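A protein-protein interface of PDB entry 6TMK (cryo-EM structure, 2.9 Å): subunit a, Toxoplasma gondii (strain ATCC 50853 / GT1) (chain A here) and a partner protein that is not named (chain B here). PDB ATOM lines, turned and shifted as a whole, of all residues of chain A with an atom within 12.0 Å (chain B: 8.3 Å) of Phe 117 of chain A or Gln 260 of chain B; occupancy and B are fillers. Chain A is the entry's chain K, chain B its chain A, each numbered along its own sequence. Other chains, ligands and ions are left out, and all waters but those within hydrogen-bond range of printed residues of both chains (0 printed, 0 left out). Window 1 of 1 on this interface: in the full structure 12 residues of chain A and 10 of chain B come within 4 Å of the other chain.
N of Ser 113 of chain A lies within hydrogen-bond range of OE2 of Glu 419 of chain B (3.0 Å).
The backbone carbonyl oxygen (O) of Pro 109 of chain A lies close to the backbone carbonyl oxygen (O) of Glu 419 of chain B (2.8 Å).
O of Ala 263 of chain B lies close to ND2 of Asn 267 of chain B, 3.4 Å away.
The indole nitrogen (NE1) of Trp 259 of chain B lies close to the side-chain amide oxygen (OE1) of Gln 260 of chain B.
CA of Gly 110 of chain A touches OE1 of Glu 419 of chain B, at 3.4 Å.
Gly 112 of chain A touches Glu 419 of chain B (C to OE2, 3.5 Å).
ND2 of Asn 267 of chain B touches NE2 of Gln 116 of chain A, 3.7 Å away.
CZ of Phe 117 of chain A touches O of Gln 260 of chain B (3.5 Å).
CE1 of Phe 117 of chain A touches CB of Ala 263 of chain B, 3.4 Å away.
Of the printed residues of chain B, Gly 112 of chain A touches Glu 419 (3.5 Å).
Of chain B, only Gln 260 and Ala 263 come within 4 Å of Phe 117 of chain A.
No residue of chain B comes within 4 Å of Gln 118 of chain A.
Thr 119 of chain A touches none of the printed residues of chain B.
Tyr 241 of chain B touches none of the printed residues of chain A.
No residue of chain A comes within 4 Å of Pro 258 of chain B.
No residue of chain A comes within 4 Å of Trp 259 of chain B.
Gln 260 of chain B touches just one residue of chain A: Phe 117.
Leu 262 of chain B touches none of the printed residues of chain A.
Ala 263 of chain B touches one residue of chain A.
No residue of chain A comes within 4 Å of His 264 of chain B.
Of the printed residues of chain A, Asn 267 of chain B touches Gln 116 (3.7 Å).
The nearest residue of chain B that does not touch Phe 117 of chain A is Trp 259 of chain B (4.04 Å).
Of the 15 printed residues of chain A, 6 touch a printed residue of chain B.
Hydrophobic or aromatic side chains of chain A that line the printed part of chain B: Pro 109 and Phe 117.
Among the printed residues, 7 pairs touch across the chains.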
ATOM      1  N   PRO A 109     -22.117  21.128  20.519  1.00  0.00           N
ATOM      2  CA  PRO A 109     -21.813  21.515  21.903  1.00  0.00           C
ATOM      3  C   PRO A 109     -21.231  20.384  22.735  1.00  0.00           C
ATOM      4  O   PRO A 109     -20.140  20.521  23.297  1.00  0.00           O
ATOM      5  CB  PRO A 109     -23.177  21.964  22.449  1.00  0.00           C
ATOM      6  CG  PRO A 109     -24.178  21.356  21.538  1.00  0.00           C
ATOM      7  CD  PRO A 109     -23.537  21.339  20.197  1.00  0.00           C
ATOM      8  N   GLY A 110     -21.943  19.264  22.822  1.00  0.00           N
ATOM      9  CA  GLY A 110     -21.584  18.183  23.713  1.00  0.00           C
ATOM     10  C   GLY A 110     -20.773  17.064  23.098  1.00  0.00           C
ATOM     11  O   GLY A 110     -20.580  16.033  23.753  1.00  0.00           O
ATOM     12  N   GLN A 111     -20.291  17.225  21.863  1.00  0.00           N
ATOM     13  CA  GLN A 111     -19.535  16.153  21.229  1.00  0.00           C
ATOM     14  C   GLN A 111     -18.222  15.892  21.954  1.00  0.00           C
ATOM     15  O   GLN A 111     -17.767  14.744  22.017  1.00  0.00           O
ATOM     16  CB  GLN A 111     -19.279  16.490  19.761  1.00  0.00           C
ATOM     17  CG  GLN A 111     -18.435  17.730  19.542  1.00  0.00           C
ATOM     18  CD  GLN A 111     -18.324  18.102  18.078  1.00  0.00           C
ATOM     19  OE1 GLN A 111     -18.973  17.500  17.223  1.00  0.00           O
ATOM     20  NE2 GLN A 111     -17.500  19.098  17.779  1.00  0.00           N
ATOM     21  N   GLY A 112     -17.621  16.929  22.540  1.00  0.00           N
ATOM     22  CA  GLY A 112     -16.378  16.735  23.267  1.00  0.00           C
ATOM     23  C   GLY A 112     -16.545  15.816  24.461  1.00  0.00           C
ATOM     24  O   GLY A 112     -15.661  15.014  24.769  1.00  0.00           O
ATOM     25  N   SER A 113     -17.681  15.924  25.149  1.00  0.00           N
ATOM     26  CA  SER A 113     -17.962  15.057  26.287  1.00  0.00           C
ATOM     27  C   SER A 113     -18.452  13.686  25.835  1.00  0.00           C
ATOM     28  O   SER A 113     -18.068  12.666  26.417  1.00  0.00           O
ATOM     29  CB  SER A 113     -18.991  15.717  27.203  1.00  0.00           C
ATOM     30  OG  SER A 113     -19.561  14.777  28.095  1.00  0.00           O
ATOM     31  N   ASN A 114     -19.292  13.639  24.800  1.00  0.00           N
ATOM     32  CA  ASN A 114     -19.856  12.382  24.327  1.00  0.00           C
ATOM     33  C   ASN A 114     -18.866  11.545  23.528  1.00  0.00           C
ATOM     34  O   ASN A 114     -19.165  10.386  23.223  1.00  0.00           O
ATOM     35  CB  ASN A 114     -21.092  12.654  23.470  1.00  0.00           C
ATOM     36  CG  ASN A 114     -22.320  12.965  24.300  1.00  0.00           C
ATOM     37  OD1 ASN A 114     -22.242  13.096  25.522  1.00  0.00           O
ATOM     38  ND2 ASN A 114     -23.465  13.085  23.638  1.00  0.00           N
ATOM     39  N   ALA A 115     -17.701  12.096  23.182  1.00  0.00           N
ATOM     40  CA  ALA A 115     -16.631  11.277  22.624  1.00  0.00           C
ATOM     41  C   ALA A 115     -15.910  10.480  23.701  1.00  0.00           C
ATOM     42  O   ALA A 115     -15.372   9.404  23.416  1.00  0.00           O
ATOM     43  CB  ALA A 115     -15.634  12.159  21.878  1.00  0.00           C
ATOM     44  N   GLN A 116     -15.884  10.990  24.932  1.00  0.00           N
ATOM     45  CA  GLN A 116     -15.237  10.286  26.031  1.00  0.00           C
ATOM     46  C   GLN A 116     -16.004   9.042  26.460  1.00  0.00           C
ATOM     47  O   GLN A 116     -15.434   8.185  27.143  1.00  0.00           O
ATOM     48  CB  GLN A 116     -15.064  11.225  27.224  1.00  0.00           C
ATOM     49  CG  GLN A 116     -13.906  12.190  27.076  1.00  0.00           C
ATOM     50  CD  GLN A 116     -12.591  11.590  27.528  1.00  0.00           C
ATOM     51  OE1 GLN A 116     -11.941  10.858  26.782  1.00  0.00           O
ATOM     52  NE2 GLN A 116     -12.192  11.897  28.756  1.00  0.00           N
ATOM     53  N   PHE A 117     -17.275   8.920  26.077  1.00  0.00           N
ATOM     54  CA  PHE A 117     -18.131   7.825  26.533  1.00  0.00           C
ATOM     55  C   PHE A 117     -18.111   6.714  25.487  1.00  0.00           C
ATOM     56  O   PHE A 117     -18.997   6.593  24.642  1.00  0.00           O
ATOM     57  CB  PHE A 117     -19.550   8.323  26.790  1.00  0.00           C
ATOM     58  CG  PHE A 117     -19.623   9.516  27.695  1.00  0.00           C
ATOM     59  CD1 PHE A 117     -18.706   9.688  28.715  1.00  0.00           C
ATOM     60  CD2 PHE A 117     -20.611  10.467  27.525  1.00  0.00           C
ATOM     61  CE1 PHE A 117     -18.774  10.787  29.544  1.00  0.00           C
ATOM     62  CE2 PHE A 117     -20.683  11.565  28.352  1.00  0.00           C
ATOM     63  CZ  PHE A 117     -19.762  11.724  29.362  1.00  0.00           C
ATOM     64  N   GLN A 118     -17.066   5.892  25.555  1.00  0.00           N
ATOM     65  CA  GLN A 118     -16.933   4.711  24.714  1.00  0.00           C
ATOM     66  C   GLN A 118     -16.484   3.549  25.585  1.00  0.00           C
ATOM     67  O   GLN A 118     -15.469   3.647  26.281  1.00  0.00           O
ATOM     68  CB  GLN A 118     -15.933   4.945  23.577  1.00  0.00           C
ATOM     69  CG  GLN A 118     -16.210   6.193  22.754  1.00  0.00           C
ATOM     70  CD  GLN A 118     -17.422   6.046  21.854  1.00  0.00           C
ATOM     71  OE1 GLN A 118     -18.330   5.265  22.136  1.00  0.00           O
ATOM     72  NE2 GLN A 118     -17.443   6.804  20.766  1.00  0.00           N
ATOM     73  N   THR A 119     -17.239   2.456  25.545  1.00  0.00           N
ATOM     74  CA  THR A 119     -17.137   1.394  26.532  1.00  0.00           C
ATOM     75  C   THR A 119     -16.651   0.105  25.879  1.00  0.00           C
ATOM     76  O   THR A 119     -16.639  -0.039  24.655  1.00  0.00           O
ATOM     77  CB  THR A 119     -18.489   1.158  27.216  1.00  0.00           C
ATOM     78  OG1 THR A 119     -19.478   0.844  26.229  1.00  0.00           O
ATOM     79  CG2 THR A 119     -18.918   2.398  27.978  1.00  0.00           C
ATOM     80  N   SER A 120     -16.249  -0.835  26.727  1.00  0.00           N
ATOM     81  CA  SER A 120     -15.891  -2.179  26.302  1.00  0.00           C
ATOM     82  C   SER A 120     -17.124  -3.072  26.229  1.00  0.00           C
ATOM     83  O   SER A 120     -18.171  -2.789  26.819  1.00  0.00           O
ATOM     84  CB  SER A 120     -14.863  -2.787  27.257  1.00  0.00           C
ATOM     85  OG  SER A 120     -14.786  -4.192  27.092  1.00  0.00           O
ATOM     86  N   LEU A 121     -16.981  -4.174  25.490  1.00  0.00           N
ATOM     87  CA  LEU A 121     -17.999  -5.220  25.510  1.00  0.00           C
ATOM     88  C   LEU A 121     -18.241  -5.718  26.929  1.00  0.00           C
ATOM     89  O   LEU A 121     -19.390  -5.859  27.365  1.00  0.00           O
ATOM     90  CB  LEU A 121     -17.574  -6.372  24.598  1.00  0.00           C
ATOM     91  CG  LEU A 121     -18.614  -7.462  24.315  1.00  0.00           C
ATOM     92  CD1 LEU A 121     -18.343  -8.100  22.963  1.00  0.00           C
ATOM     93  CD2 LEU A 121     -18.632  -8.524  25.404  1.00  0.00           C
ATOM     94  N   ASP A 123     -17.503  -4.117  29.685  1.00  0.00           N
ATOM     95  CA  ASP A 123     -18.089  -2.999  30.418  1.00  0.00           C
ATOM     96  C   ASP A 123     -19.602  -2.972  30.248  1.00  0.00           C
ATOM     97  O   ASP A 123     -20.351  -2.852  31.226  1.00  0.00           O
ATOM     98  CB  ASP A 123     -17.472  -1.682  29.948  1.00  0.00           C
ATOM     99  CG  ASP A 123     -16.181  -1.344  30.675  1.00  0.00           C
ATOM    100  OD1 ASP A 123     -15.979  -1.838  31.805  1.00  0.00           O
ATOM    101  OD2 ASP A 123     -15.367  -0.581  30.113  1.00  0.00           O
ATOM    102  N   LYS A 124     -20.074  -3.088  29.007  1.00  0.00           N
ATOM    103  CA  LYS A 124     -21.503  -2.965  28.764  1.00  0.00           C
ATOM    104  C   LYS A 124     -22.258  -4.216  29.193  1.00  0.00           C
ATOM    105  O   LYS A 124     -23.422  -4.118  29.591  1.00  0.00           O
ATOM    106  CB  LYS A 124     -21.760  -2.654  27.290  1.00  0.00           C
ATOM    107  CG  LYS A 124     -21.431  -3.779  26.331  1.00  0.00           C
ATOM    108  CD  LYS A 124     -21.728  -3.368  24.897  1.00  0.00           C
ATOM    109  CE  LYS A 124     -20.689  -2.390  24.368  1.00  0.00           C
ATOM    110  NZ  LYS A 124     -20.978  -1.947  22.976  1.00  0.00           N
ATOM    111  N   TYR B 241     -20.370  23.150  37.766  1.00  0.00           N
ATOM    112  CA  TYR B 241     -20.485  22.557  36.441  1.00  0.00           C
ATOM    113  C   TYR B 241     -21.734  23.058  35.734  1.00  0.00           C
ATOM    114  O   TYR B 241     -21.714  23.317  34.525  1.00  0.00           O
ATOM    115  CB  TYR B 241     -20.498  21.036  36.553  1.00  0.00           C
ATOM    116  CG  TYR B 241     -20.295  20.327  35.240  1.00  0.00           C
ATOM    117  CD1 TYR B 241     -19.029  19.964  34.822  1.00  0.00           C
ATOM    118  CD2 TYR B 241     -21.360  20.031  34.415  1.00  0.00           C
ATOM    119  CE1 TYR B 241     -18.832  19.324  33.626  1.00  0.00           C
ATOM    120  CE2 TYR B 241     -21.170  19.389  33.215  1.00  0.00           C
ATOM    121  CZ  TYR B 241     -19.905  19.041  32.825  1.00  0.00           C
ATOM    122  OH  TYR B 241     -19.711  18.397  31.628  1.00  0.00           O
ATOM    123  N   ARG B 245     -21.266  24.784  32.285  1.00  0.00           N
ATOM    124  CA  ARG B 245     -21.756  24.022  31.145  1.00  0.00           C
ATOM    125  C   ARG B 245     -22.962  24.697  30.515  1.00  0.00           C
ATOM    126  O   ARG B 245     -23.150  24.630  29.295  1.00  0.00           O
ATOM    127  CB  ARG B 245     -22.105  22.602  31.588  1.00  0.00           C
ATOM    128  CG  ARG B 245     -22.777  21.740  30.539  1.00  0.00           C
ATOM    129  CD  ARG B 245     -21.955  21.615  29.284  1.00  0.00           C
ATOM    130  NE  ARG B 245     -22.547  20.671  28.344  1.00  0.00           N
ATOM    131  CZ  ARG B 245     -22.523  19.352  28.501  1.00  0.00           C
ATOM    132  NH1 ARG B 245     -23.085  18.567  27.597  1.00  0.00           N
ATOM    133  NH2 ARG B 245     -21.944  18.817  29.561  1.00  0.00           N
ATOM    134  N   PRO B 257     -28.951  15.689  38.314  1.00  0.00           N
ATOM    135  CA  PRO B 257     -28.132  16.004  37.148  1.00  0.00           C
ATOM    136  C   PRO B 257     -28.126  14.859  36.154  1.00  0.00           C
ATOM    137  O   PRO B 257     -28.513  13.729  36.489  1.00  0.00           O
ATOM    138  CB  PRO B 257     -26.734  16.231  37.743  1.00  0.00           C
ATOM    139  CG  PRO B 257     -26.907  16.204  39.208  1.00  0.00           C
ATOM    140  CD  PRO B 257     -28.107  15.392  39.477  1.00  0.00           C
ATOM    141  N   PRO B 258     -27.694  15.106  34.922  1.00  0.00           N
ATOM    142  CA  PRO B 258     -27.495  14.010  33.973  1.00  0.00           C
ATOM    143  C   PRO B 258     -26.234  13.191  34.206  1.00  0.00           C
ATOM    144  O   PRO B 258     -25.204  13.670  34.698  1.00  0.00           O
ATOM    145  CB  PRO B 258     -27.433  14.727  32.621  1.00  0.00           C
ATOM    146  CG  PRO B 258     -28.123  15.998  32.831  1.00  0.00           C
ATOM    147  CD  PRO B 258     -27.843  16.393  34.231  1.00  0.00           C
ATOM    148  N   TRP B 259     -26.339  11.922  33.811  1.00  0.00           N
ATOM    149  CA  TRP B 259     -25.217  11.003  33.927  1.00  0.00           C
ATOM    150  C   TRP B 259     -24.050  11.450  33.066  1.00  0.00           C
ATOM    151  O   TRP B 259     -22.893  11.181  33.400  1.00  0.00           O
ATOM    152  CB  TRP B 259     -25.660   9.591  33.552  1.00  0.00           C
ATOM    153  CG  TRP B 259     -26.117   9.440  32.142  1.00  0.00           C
ATOM    154  CD1 TRP B 259     -27.383   9.588  31.675  1.00  0.00           C
ATOM    155  CD2 TRP B 259     -25.310   9.095  31.013  1.00  0.00           C
ATOM    156  NE1 TRP B 259     -27.420   9.362  30.324  1.00  0.00           N
ATOM    157  CE2 TRP B 259     -26.157   9.057  29.894  1.00  0.00           C
ATOM    158  CE3 TRP B 259     -23.954   8.815  30.841  1.00  0.00           C
ATOM    159  CZ2 TRP B 259     -25.694   8.754  28.621  1.00  0.00           C
ATOM    160  CZ3 TRP B 259     -23.498   8.518  29.580  1.00  0.00           C
ATOM    161  CH2 TRP B 259     -24.363   8.489  28.486  1.00  0.00           C
ATOM    162  N   GLN B 260     -24.328  12.144  31.962  1.00  0.00           N
ATOM    163  CA  GLN B 260     -23.253  12.696  31.150  1.00  0.00           C
ATOM    164  C   GLN B 260     -22.440  13.698  31.954  1.00  0.00           C
ATOM    165  O   GLN B 260     -21.203  13.664  31.958  1.00  0.00           O
ATOM    166  CB  GLN B 260     -23.841  13.370  29.915  1.00  0.00           C
ATOM    167  CG  GLN B 260     -24.625  12.453  29.013  1.00  0.00           C
ATOM    168  CD  GLN B 260     -26.097  12.448  29.339  1.00  0.00           C
ATOM    169  OE1 GLN B 260     -26.492  12.675  30.479  1.00  0.00           O
ATOM    170  NE2 GLN B 260     -26.920  12.188  28.336  1.00  0.00           N
ATOM    171  N   TRP B 261     -23.131  14.603  32.643  1.00  0.00           N
ATOM    172  CA  TRP B 261     -22.452  15.580  33.478  1.00  0.00           C
ATOM    173  C   TRP B 261     -21.654  14.894  34.574  1.00  0.00           C
ATOM    174  O   TRP B 261     -20.511  15.274  34.856  1.00  0.00           O
ATOM    175  CB  TRP B 261     -23.471  16.526  34.097  1.00  0.00           C
ATOM    176  CG  TRP B 261     -24.175  17.384  33.113  1.00  0.00           C
ATOM    177  CD1 TRP B 261     -24.214  17.219  31.768  1.00  0.00           C
ATOM    178  CD2 TRP B 261     -24.957  18.542  33.399  1.00  0.00           C
ATOM    179  NE1 TRP B 261     -24.970  18.204  31.192  1.00  0.00           N
ATOM    180  CE2 TRP B 261     -25.439  19.030  32.176  1.00  0.00           C
ATOM    181  CE3 TRP B 261     -25.299  19.213  34.573  1.00  0.00           C
ATOM    182  CZ2 TRP B 261     -26.239  20.157  32.090  1.00  0.00           C
ATOM    183  CZ3 TRP B 261     -26.092  20.331  34.486  1.00  0.00           C
ATOM    184  CH2 TRP B 261     -26.555  20.793  33.254  1.00  0.00           C
ATOM    185  N   LEU B 262     -22.243  13.878  35.205  1.00  0.00           N
ATOM    186  CA  LEU B 262     -21.536  13.185  36.277  1.00  0.00           C
ATOM    187  C   LEU B 262     -20.273  12.505  35.761  1.00  0.00           C
ATOM    188  O   LEU B 262     -19.211  12.577  36.393  1.00  0.00           O
ATOM    189  CB  LEU B 262     -22.468  12.177  36.939  1.00  0.00           C
ATOM    190  CG  LEU B 262     -23.559  12.809  37.802  1.00  0.00           C
ATOM    191  CD1 LEU B 262     -24.676  11.836  38.068  1.00  0.00           C
ATOM    192  CD2 LEU B 262     -22.985  13.301  39.101  1.00  0.00           C
ATOM    193  N   ALA B 263     -20.371  11.834  34.614  1.00  0.00           N
ATOM    194  CA  ALA B 263     -19.210  11.163  34.046  1.00  0.00           C
ATOM    195  C   ALA B 263     -18.120  12.160  33.683  1.00  0.00           C
ATOM    196  O   ALA B 263     -16.931  11.911  33.920  1.00  0.00           O
ATOM    197  CB  ALA B 263     -19.634  10.364  32.819  1.00  0.00           C
ATOM    198  N   HIS B 264     -18.505  13.287  33.084  1.00  0.00           N
ATOM    199  CA  HIS B 264     -17.525  14.321  32.779  1.00  0.00           C
ATOM    200  C   HIS B 264     -16.846  14.820  34.048  1.00  0.00           C
ATOM    201  O   HIS B 264     -15.630  15.051  34.066  1.00  0.00           O
ATOM    202  CB  HIS B 264     -18.210  15.463  32.037  1.00  0.00           C
ATOM    203  CG  HIS B 264     -17.265  16.379  31.329  1.00  0.00           C
ATOM    204  ND1 HIS B 264     -17.535  17.714  31.130  1.00  0.00           N
ATOM    205  CD2 HIS B 264     -16.057  16.151  30.765  1.00  0.00           C
ATOM    206  CE1 HIS B 264     -16.532  18.270  30.476  1.00  0.00           C
ATOM    207  NE2 HIS B 264     -15.622  17.343  30.242  1.00  0.00           N
ATOM    208  N   MET B 265     -17.618  14.991  35.122  1.00  0.00           N
ATOM    209  CA  MET B 265     -17.030  15.406  36.389  1.00  0.00           C
ATOM    210  C   MET B 265     -16.006  14.394  36.873  1.00  0.00           C
ATOM    211  O   MET B 265     -14.935  14.767  37.362  1.00  0.00           O
ATOM    212  CB  MET B 265     -18.109  15.576  37.451  1.00  0.00           C
ATOM    213  CG  MET B 265     -18.931  16.829  37.339  1.00  0.00           C
ATOM    214  SD  MET B 265     -20.224  16.849  38.590  1.00  0.00           S
ATOM    215  CE  MET B 265     -21.582  17.527  37.658  1.00  0.00           C
ATOM    216  N   GLU B 266     -16.326  13.105  36.764  1.00  0.00           N
ATOM    217  CA  GLU B 266     -15.384  12.085  37.213  1.00  0.00           C
ATOM    218  C   GLU B 266     -14.117  12.084  36.369  1.00  0.00           C
ATOM    219  O   GLU B 266     -13.016  11.883  36.892  1.00  0.00           O
ATOM    220  CB  GLU B 266     -16.045  10.710  37.181  1.00  0.00           C
ATOM    221  CG  GLU B 266     -17.262  10.573  38.077  1.00  0.00           C
ATOM    222  CD  GLU B 266     -17.059  11.182  39.448  1.00  0.00           C
ATOM    223  OE1 GLU B 266     -15.965  11.004  40.022  1.00  0.00           O
ATOM    224  OE2 GLU B 266     -17.992  11.842  39.951  1.00  0.00           O
ATOM    225  N   ASN B 267     -14.246  12.308  35.062  1.00  0.00           N
ATOM    226  CA  ASN B 267     -13.056  12.384  34.219  1.00  0.00           C
ATOM    227  C   ASN B 267     -12.174  13.566  34.609  1.00  0.00           C
ATOM    228  O   ASN B 267     -10.942  13.441  34.698  1.00  0.00           O
ATOM    229  CB  ASN B 267     -13.464  12.479  32.752  1.00  0.00           C
ATOM    230  CG  ASN B 267     -14.208  11.251  32.280  1.00  0.00           C
ATOM    231  OD1 ASN B 267     -14.091  10.178  32.869  1.00  0.00           O
ATOM    232  ND2 ASN B 267     -14.977  11.400  31.211  1.00  0.00           N
ATOM    233  N   GLU B 419     -17.742  23.028  25.995  1.00  0.00           N
ATOM    234  CA  GLU B 419     -18.935  22.189  25.918  1.00  0.00           C
ATOM    235  C   GLU B 419     -20.184  22.982  25.554  1.00  0.00           C
ATOM    236  O   GLU B 419     -21.182  22.382  25.140  1.00  0.00           O
ATOM    237  CB  GLU B 419     -19.160  21.459  27.241  1.00  0.00           C
ATOM    238  CG  GLU B 419     -18.104  20.426  27.563  1.00  0.00           C
ATOM    239  CD  GLU B 419     -18.091  19.285  26.566  1.00  0.00           C
ATOM    240  OE1 GLU B 419     -19.120  19.073  25.892  1.00  0.00           O
ATOM    241  OE2 GLU B 419     -17.052  18.601  26.455  1.00  0.00           O
